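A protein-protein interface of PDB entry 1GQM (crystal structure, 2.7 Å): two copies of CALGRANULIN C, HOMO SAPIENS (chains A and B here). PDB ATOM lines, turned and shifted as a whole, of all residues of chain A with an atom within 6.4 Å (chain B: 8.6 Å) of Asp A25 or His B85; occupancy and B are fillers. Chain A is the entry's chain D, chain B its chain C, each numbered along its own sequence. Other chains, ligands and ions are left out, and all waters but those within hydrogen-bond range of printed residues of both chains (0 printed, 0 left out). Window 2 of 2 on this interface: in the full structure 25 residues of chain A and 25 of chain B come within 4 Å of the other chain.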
ATOM      1  N   LEU A   7      -5.947 -24.180  19.174  1.00  0.00           N
ATOM      2  CA  LEU A   7      -6.030 -24.100  20.645  1.00  0.00           C
ATOM      3  C   LEU A   7      -5.500 -22.771  21.186  1.00  0.00           C
ATOM      4  O   LEU A   7      -6.138 -22.097  21.963  1.00  0.00           O
ATOM      5  CB  LEU A   7      -5.331 -25.297  21.304  1.00  0.00           C
ATOM      6  CG  LEU A   7      -6.031 -26.635  20.968  1.00  0.00           C
ATOM      7  CD1 LEU A   7      -5.406 -27.807  21.660  1.00  0.00           C
ATOM      8  CD2 LEU A   7      -7.558 -26.601  21.208  1.00  0.00           C
ATOM      9  N   VAL A  11      -7.497 -19.611  23.144  1.00  0.00           N
ATOM     10  CA  VAL A  11      -6.991 -19.030  24.375  1.00  0.00           C
ATOM     11  C   VAL A  11      -6.829 -17.537  24.187  1.00  0.00           C
ATOM     12  O   VAL A  11      -7.270 -16.734  25.026  1.00  0.00           O
ATOM     13  CB  VAL A  11      -5.701 -19.734  24.835  1.00  0.00           C
ATOM     14  CG1 VAL A  11      -4.962 -18.918  25.885  1.00  0.00           C
ATOM     15  CG2 VAL A  11      -6.064 -21.069  25.403  1.00  0.00           C
ATOM     16  N   PHE A  14     -10.057 -15.678  24.343  1.00  0.00           N
ATOM     17  CA  PHE A  14     -10.524 -15.548  25.722  1.00  0.00           C
ATOM     18  C   PHE A  14      -9.974 -14.275  26.291  1.00  0.00           C
ATOM     19  O   PHE A  14     -10.715 -13.420  26.737  1.00  0.00           O
ATOM     20  CB  PHE A  14     -10.013 -16.722  26.557  1.00  0.00           C
ATOM     21  CG  PHE A  14     -10.517 -16.752  27.965  1.00  0.00           C
ATOM     22  CD1 PHE A  14     -11.847 -17.085  28.243  1.00  0.00           C
ATOM     23  CD2 PHE A  14      -9.650 -16.465  29.032  1.00  0.00           C
ATOM     24  CE1 PHE A  14     -12.282 -17.123  29.570  1.00  0.00           C
ATOM     25  CE2 PHE A  14     -10.078 -16.501  30.355  1.00  0.00           C
ATOM     26  CZ  PHE A  14     -11.371 -16.833  30.630  1.00  0.00           C
ATOM     27  N   HIS A  15      -8.660 -14.140  26.261  1.00  0.00           N
ATOM     28  CA  HIS A  15      -8.032 -12.963  26.846  1.00  0.00           C
ATOM     29  C   HIS A  15      -8.369 -11.705  26.144  1.00  0.00           C
ATOM     30  O   HIS A  15      -8.453 -10.650  26.735  1.00  0.00           O
ATOM     31  CB  HIS A  15      -6.539 -13.135  26.966  1.00  0.00           C
ATOM     32  CG  HIS A  15      -6.189 -14.142  27.998  1.00  0.00           C
ATOM     33  ND1 HIS A  15      -5.313 -15.178  27.773  1.00  0.00           N
ATOM     34  CD2 HIS A  15      -6.687 -14.329  29.238  1.00  0.00           C
ATOM     35  CE1 HIS A  15      -5.270 -15.951  28.842  1.00  0.00           C
ATOM     36  NE2 HIS A  15      -6.092 -15.456  29.746  1.00  0.00           N
ATOM     37  N   SER A  18     -11.245 -10.834  28.102  1.00  0.00           N
ATOM     38  CA  SER A  18     -11.182 -10.785  29.552  1.00  0.00           C
ATOM     39  C   SER A  18     -10.455  -9.587  30.115  1.00  0.00           C
ATOM     40  O   SER A  18     -10.634  -9.234  31.296  1.00  0.00           O
ATOM     41  CB  SER A  18     -10.634 -12.091  30.136  1.00  0.00           C
ATOM     42  OG  SER A  18      -9.449 -12.504  29.473  1.00  0.00           O
ATOM     43  N   VAL A  19      -9.644  -8.945  29.289  1.00  0.00           N
ATOM     44  CA  VAL A  19      -8.892  -7.789  29.759  1.00  0.00           C
ATOM     45  C   VAL A  19      -9.641  -6.470  29.722  1.00  0.00           C
ATOM     46  O   VAL A  19      -9.194  -5.507  30.342  1.00  0.00           O
ATOM     47  CB  VAL A  19      -7.651  -7.528  28.927  1.00  0.00           C
ATOM     48  CG1 VAL A  19      -6.431  -8.234  29.515  1.00  0.00           C
ATOM     49  CG2 VAL A  19      -7.914  -7.865  27.461  1.00  0.00           C
ATOM     50  N   GLY A  22     -12.305  -5.147  34.811  1.00  0.00           N
ATOM     51  CA  GLY A  22     -12.091  -5.927  36.011  1.00  0.00           C
ATOM     52  C   GLY A  22     -10.889  -6.836  35.914  1.00  0.00           C
ATOM     53  O   GLY A  22      -9.869  -6.431  35.347  1.00  0.00           O
ATOM     54  N   HIS A  23     -11.005  -8.049  36.461  1.00  0.00           N
ATOM     55  CA  HIS A  23      -9.908  -9.018  36.436  1.00  0.00           C
ATOM     56  C   HIS A  23      -9.491  -9.327  35.004  1.00  0.00           C
ATOM     57  O   HIS A  23     -10.329  -9.496  34.118  1.00  0.00           O
ATOM     58  CB  HIS A  23     -10.255 -10.282  37.228  1.00  0.00           C
ATOM     59  N   PHE A  24      -8.193  -9.373  34.764  1.00  0.00           N
ATOM     60  CA  PHE A  24      -7.734  -9.549  33.403  1.00  0.00           C
ATOM     61  C   PHE A  24      -7.911 -10.971  32.937  1.00  0.00           C
ATOM     62  O   PHE A  24      -8.171 -11.184  31.760  1.00  0.00           O
ATOM     63  CB  PHE A  24      -6.303  -9.057  33.246  1.00  0.00           C
ATOM     64  CG  PHE A  24      -6.107  -7.641  33.727  1.00  0.00           C
ATOM     65  CD1 PHE A  24      -7.134  -6.718  33.632  1.00  0.00           C
ATOM     66  CD2 PHE A  24      -4.892  -7.229  34.272  1.00  0.00           C
ATOM     67  CE1 PHE A  24      -6.949  -5.400  34.061  1.00  0.00           C
ATOM     68  CE2 PHE A  24      -4.697  -5.907  34.712  1.00  0.00           C
ATOM     69  CZ  PHE A  24      -5.718  -4.992  34.613  1.00  0.00           C
ATOM     70  N   ASP A  25      -7.808 -11.956  33.834  1.00  0.00           N
ATOM     71  CA  ASP A  25      -7.976 -13.357  33.397  1.00  0.00           C
ATOM     72  C   ASP A  25      -9.379 -13.838  33.532  1.00  0.00           C
ATOM     73  O   ASP A  25      -9.599 -15.028  33.438  1.00  0.00           O
ATOM     74  CB  ASP A  25      -7.076 -14.361  34.155  1.00  0.00           C
ATOM     75  CG  ASP A  25      -7.313 -15.884  33.691  1.00  0.00           C
ATOM     76  OD1 ASP A  25      -8.346 -16.545  34.116  1.00  0.00           O
ATOM     77  OD2 ASP A  25      -6.482 -16.494  32.917  1.00  0.00           O
ATOM     78  N   THR A  26     -10.333 -12.960  33.799  1.00  0.00           N
ATOM     79  CA  THR A  26     -11.707 -13.455  33.907  1.00  0.00           C
ATOM     80  C   THR A  26     -12.727 -12.560  33.255  1.00  0.00           C
ATOM     81  O   THR A  26     -12.562 -11.325  33.247  1.00  0.00           O
ATOM     82  CB  THR A  26     -12.125 -13.643  35.339  1.00  0.00           C
ATOM     83  OG1 THR A  26     -12.173 -12.359  35.963  1.00  0.00           O
ATOM     84  CG2 THR A  26     -11.057 -14.428  36.124  1.00  0.00           C
ATOM     85  N   LEU A  27     -13.804 -13.193  32.764  1.00  0.00           N
ATOM     86  CA  LEU A  27     -14.824 -12.518  32.000  1.00  0.00           C
ATOM     87  C   LEU A  27     -15.962 -12.149  32.859  1.00  0.00           C
ATOM     88  O   LEU A  27     -16.511 -13.019  33.592  1.00  0.00           O
ATOM     89  CB  LEU A  27     -15.387 -13.440  30.950  1.00  0.00           C
ATOM     90  CG  LEU A  27     -14.635 -13.851  29.694  1.00  0.00           C
ATOM     91  CD1 LEU A  27     -15.294 -15.115  29.118  1.00  0.00           C
ATOM     92  CD2 LEU A  27     -14.552 -12.735  28.668  1.00  0.00           C
ATOM     93  N   VAL A  68     -16.460 -15.403  34.902  1.00  0.00           N
ATOM     94  CA  VAL A  68     -16.231 -16.655  34.198  1.00  0.00           C
ATOM     95  C   VAL A  68     -14.739 -16.905  33.984  1.00  0.00           C
ATOM     96  O   VAL A  68     -14.167 -16.291  33.094  1.00  0.00           O
ATOM     97  CB  VAL A  68     -16.813 -16.667  32.788  1.00  0.00           C
ATOM     98  CG1 VAL A  68     -16.384 -17.943  32.132  1.00  0.00           C
ATOM     99  CG2 VAL A  68     -18.270 -16.669  32.806  1.00  0.00           C
ATOM    100  N   ASP A  69     -14.108 -17.814  34.734  1.00  0.00           N
ATOM    101  CA  ASP A  69     -12.651 -18.039  34.542  1.00  0.00           C
ATOM    102  C   ASP A  69     -12.371 -19.006  33.416  1.00  0.00           C
ATOM    103  O   ASP A  69     -13.288 -19.571  32.825  1.00  0.00           O
ATOM    104  CB  ASP A  69     -11.895 -18.464  35.835  1.00  0.00           C
ATOM    105  CG  ASP A  69     -12.394 -19.796  36.416  1.00  0.00           C
ATOM    106  OD1 ASP A  69     -13.045 -20.579  35.680  1.00  0.00           O
ATOM    107  OD2 ASP A  69     -12.213 -20.151  37.609  1.00  0.00           O
ATOM    108  N   PHE A  70     -11.091 -19.232  33.161  1.00  0.00           N
ATOM    109  CA  PHE A  70     -10.720 -20.063  32.025  1.00  0.00           C
ATOM    110  C   PHE A  70     -11.225 -21.486  32.190  1.00  0.00           C
ATOM    111  O   PHE A  70     -11.738 -22.071  31.257  1.00  0.00           O
ATOM    112  CB  PHE A  70      -9.205 -19.970  31.636  1.00  0.00           C
ATOM    113  CG  PHE A  70      -8.886 -20.706  30.358  1.00  0.00           C
ATOM    114  CD1 PHE A  70      -9.213 -20.158  29.123  1.00  0.00           C
ATOM    115  CD2 PHE A  70      -8.374 -21.998  30.385  1.00  0.00           C
ATOM    116  CE1 PHE A  70      -9.004 -20.848  27.957  1.00  0.00           C
ATOM    117  CE2 PHE A  70      -8.153 -22.680  29.201  1.00  0.00           C
ATOM    118  CZ  PHE A  70      -8.464 -22.096  28.000  1.00  0.00           C
ATOM    119  N   GLN A  71     -11.098 -22.069  33.361  1.00  0.00           N
ATOM    120  CA  GLN A  71     -11.603 -23.419  33.441  1.00  0.00           C
ATOM    121  C   GLN A  71     -13.111 -23.453  33.222  1.00  0.00           C
ATOM    122  O   GLN A  71     -13.606 -24.408  32.629  1.00  0.00           O
ATOM    123  CB  GLN A  71     -11.183 -24.174  34.698  1.00  0.00           C
ATOM    124  CG  GLN A  71     -10.479 -25.489  34.288  1.00  0.00           C
ATOM    125  CD  GLN A  71      -8.945 -25.321  34.112  1.00  0.00           C
ATOM    126  OE1 GLN A  71      -8.190 -26.302  34.136  1.00  0.00           O
ATOM    127  NE2 GLN A  71      -8.493 -24.072  33.944  1.00  0.00           N
ATOM    128  N   THR B  43       1.842 -30.362  23.140  1.00  0.00           N
ATOM    129  CA  THR B  43       0.820 -30.005  24.103  1.00  0.00           C
ATOM    130  C   THR B  43       0.646 -30.932  25.282  1.00  0.00           C
ATOM    131  O   THR B  43       0.409 -30.476  26.369  1.00  0.00           O
ATOM    132  CB  THR B  43      -0.489 -29.735  23.385  1.00  0.00           C
ATOM    133  OG1 THR B  43      -0.323 -28.544  22.575  1.00  0.00           O
ATOM    134  CG2 THR B  43      -1.537 -29.387  24.387  1.00  0.00           C
ATOM    135  N   ALA B  78     -10.899 -30.611  25.642  1.00  0.00           N
ATOM    136  CA  ALA B  78     -10.878 -30.080  26.979  1.00  0.00           C
ATOM    137  C   ALA B  78      -9.486 -30.238  27.646  1.00  0.00           C
ATOM    138  O   ALA B  78      -8.908 -29.281  28.172  1.00  0.00           O
ATOM    139  CB  ALA B  78     -11.960 -30.749  27.798  1.00  0.00           C
ATOM    140  N   ILE B  79      -8.975 -31.462  27.655  1.00  0.00           N
ATOM    141  CA  ILE B  79      -7.677 -31.733  28.228  1.00  0.00           C
ATOM    142  C   ILE B  79      -6.659 -30.852  27.552  1.00  0.00           C
ATOM    143  O   ILE B  79      -5.818 -30.276  28.226  1.00  0.00           O
ATOM    144  CB  ILE B  79      -7.261 -33.180  27.913  1.00  0.00           C
ATOM    145  CG1 ILE B  79      -8.035 -34.180  28.784  1.00  0.00           C
ATOM    146  CG2 ILE B  79      -5.760 -33.327  28.086  1.00  0.00           C
ATOM    147  CD1 ILE B  79      -8.178 -35.528  28.130  1.00  0.00           C
ATOM    148  N   ALA B  80      -6.726 -30.729  26.225  1.00  0.00           N
ATOM    149  CA  ALA B  80      -5.700 -29.967  25.549  1.00  0.00           C
ATOM    150  C   ALA B  80      -5.776 -28.487  25.857  1.00  0.00           C
ATOM    151  O   ALA B  80      -4.775 -27.856  26.186  1.00  0.00           O
ATOM    152  CB  ALA B  80      -5.761 -30.199  24.087  1.00  0.00           C
ATOM    153  N   LEU B  81      -6.970 -27.937  25.733  1.00  0.00           N
ATOM    154  CA  LEU B  81      -7.204 -26.534  25.986  1.00  0.00           C
ATOM    155  C   LEU B  81      -6.646 -26.126  27.324  1.00  0.00           C
ATOM    156  O   LEU B  81      -6.254 -24.968  27.539  1.00  0.00           O
ATOM    157  CB  LEU B  81      -8.691 -26.314  26.077  1.00  0.00           C
ATOM    158  CG  LEU B  81      -9.175 -25.673  24.822  1.00  0.00           C
ATOM    159  CD1 LEU B  81     -10.690 -25.491  24.952  1.00  0.00           C
ATOM    160  CD2 LEU B  81      -8.425 -24.341  24.701  1.00  0.00           C
ATOM    161  N   LYS B  82      -6.642 -27.078  28.241  1.00  0.00           N
ATOM    162  CA  LYS B  82      -6.265 -26.754  29.592  1.00  0.00           C
ATOM    163  C   LYS B  82      -4.855 -26.372  29.509  1.00  0.00           C
ATOM    164  O   LYS B  82      -4.453 -25.258  29.918  1.00  0.00           O
ATOM    165  CB  LYS B  82      -6.336 -27.991  30.483  1.00  0.00           C
ATOM    166  CG  LYS B  82      -6.615 -27.624  31.937  1.00  0.00           C
ATOM    167  CD  LYS B  82      -7.400 -28.758  32.604  1.00  0.00           C
ATOM    168  N   ALA B  83      -4.119 -27.357  28.969  1.00  0.00           N
ATOM    169  CA  ALA B  83      -2.681 -27.321  28.819  1.00  0.00           C
ATOM    170  C   ALA B  83      -2.232 -26.097  27.999  1.00  0.00           C
ATOM    171  O   ALA B  83      -1.296 -25.356  28.384  1.00  0.00           O
ATOM    172  CB  ALA B  83      -2.228 -28.610  28.224  1.00  0.00           C
ATOM    173  N   ALA B  84      -2.935 -25.837  26.899  1.00  0.00           N
ATOM    174  CA  ALA B  84      -2.541 -24.702  26.053  1.00  0.00           C
ATOM    175  C   ALA B  84      -2.676 -23.360  26.772  1.00  0.00           C
ATOM    176  O   ALA B  84      -1.847 -22.457  26.612  1.00  0.00           O
ATOM    177  CB  ALA B  84      -3.310 -24.687  24.747  1.00  0.00           C
ATOM    178  N   HIS B  85      -3.719 -23.207  27.553  1.00  0.00           N
ATOM    179  CA  HIS B  85      -3.814 -21.972  28.301  1.00  0.00           C
ATOM    180  C   HIS B  85      -2.690 -21.874  29.340  1.00  0.00           C
ATOM    181  O   HIS B  85      -2.244 -20.767  29.662  1.00  0.00           O
ATOM    182  CB  HIS B  85      -5.179 -21.829  28.965  1.00  0.00           C
ATOM    183  CG  HIS B  85      -5.240 -20.707  29.935  1.00  0.00           C
ATOM    184  ND1 HIS B  85      -5.469 -19.409  29.545  1.00  0.00           N
ATOM    185  CD2 HIS B  85      -5.063 -20.675  31.279  1.00  0.00           C
ATOM    186  CE1 HIS B  85      -5.448 -18.620  30.609  1.00  0.00           C
ATOM    187  NE2 HIS B  85      -5.206 -19.366  31.675  1.00  0.00           N
ATOM    188  N   TYR B  86      -2.220 -23.027  29.845  1.00  0.00           N
ATOM    189  CA  TYR B  86      -1.176 -23.024  30.908  1.00  0.00           C
ATOM    190  C   TYR B  86       0.121 -22.348  30.435  1.00  0.00           C
ATOM    191  O   TYR B  86       0.684 -21.489  31.137  1.00  0.00           O
ATOM    192  CB  TYR B  86      -0.866 -24.438  31.475  1.00  0.00           C
ATOM    193  N   HIS B  87       0.577 -22.747  29.246  1.00  0.00           N
ATOM    194  CA  HIS B  87       1.797 -22.178  28.710  1.00  0.00           C
ATOM    195  C   HIS B  87       1.656 -20.647  28.663  1.00  0.00           C
ATOM    196  O   HIS B  87       2.071 -19.941  29.596  1.00  0.00           O
ATOM    197  CB  HIS B  87       2.148 -22.775  27.333  1.00  0.00           C
ATOM    198  CG  HIS B  87       3.430 -22.239  26.754  1.00  0.00           C
ATOM    199  ND1 HIS B  87       3.458 -21.291  25.750  1.00  0.00           N
ATOM    200  CD2 HIS B  87       4.729 -22.508  27.051  1.00  0.00           C
ATOM    201  CE1 HIS B  87       4.715 -21.001  25.453  1.00  0.00           C
ATOM    202  NE2 HIS B  87       5.507 -21.726  26.229  1.00  0.00           N
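A ring nitrogen (NE2) of His B85 sits close to the side-chain carboxylate (OD2) of Asp A25, at 3.4 Å.
NE2 of His A15 lies within hydrogen-bond range of OD2 of Asp A25, at 3.4 Å. OG of Ser A18 lies close to O of His A15. The side-chain carboxylate (OD1) of Asp A69 sits close to the backbone NH (N) of Gln A71, at 3.4 Å.
Leu A7 touches Ala B80. Val A11 touches His B85 (CG1 to ND1, 3.7 Å). His A15 touches His B85. CE2 of Phe A70 touches O of Leu B81 (3.4 Å). Phe A70 touches His B85. OE1 of Gln A71 touches CD of Lys B82 (3.0 Å).
Printed residues of chain B within 4 Å of Leu A7: Ala B80 (3.4 Å). Of the printed residues of chain B, Val A11 touches His B85 (3.7 Å). Phe A14 touches none of the printed residues of chain B. Ser A18 touches none of the printed residues of chain B. No residue of chain B comes within 4 Å of Thr A26. Of the printed residues of chain A, Ala B80 touches Leu A7 (3.4 Å). Of the printed residues of chain A, Leu B81 touches Phe A70. His B85 touches just these residues of chain A: Val A11, His A15, Asp A25 and Phe A70.
Hydrophobic or aromatic side chains of chain B within 4 Å of the printed part of chain A: Ala B80, Leu B81 and His B85. Among the printed residues, 7 pairs touch across the chains. Among the printed residues, no Asp or Glu carboxylate lies within 4 Å of a Lys or Arg side-chain nitrogen of the other chain.
No position is printed for both chains. Of the 7 pairs that touch across the chains among the printed residues, none has its exchanged pair printed and touching as well.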
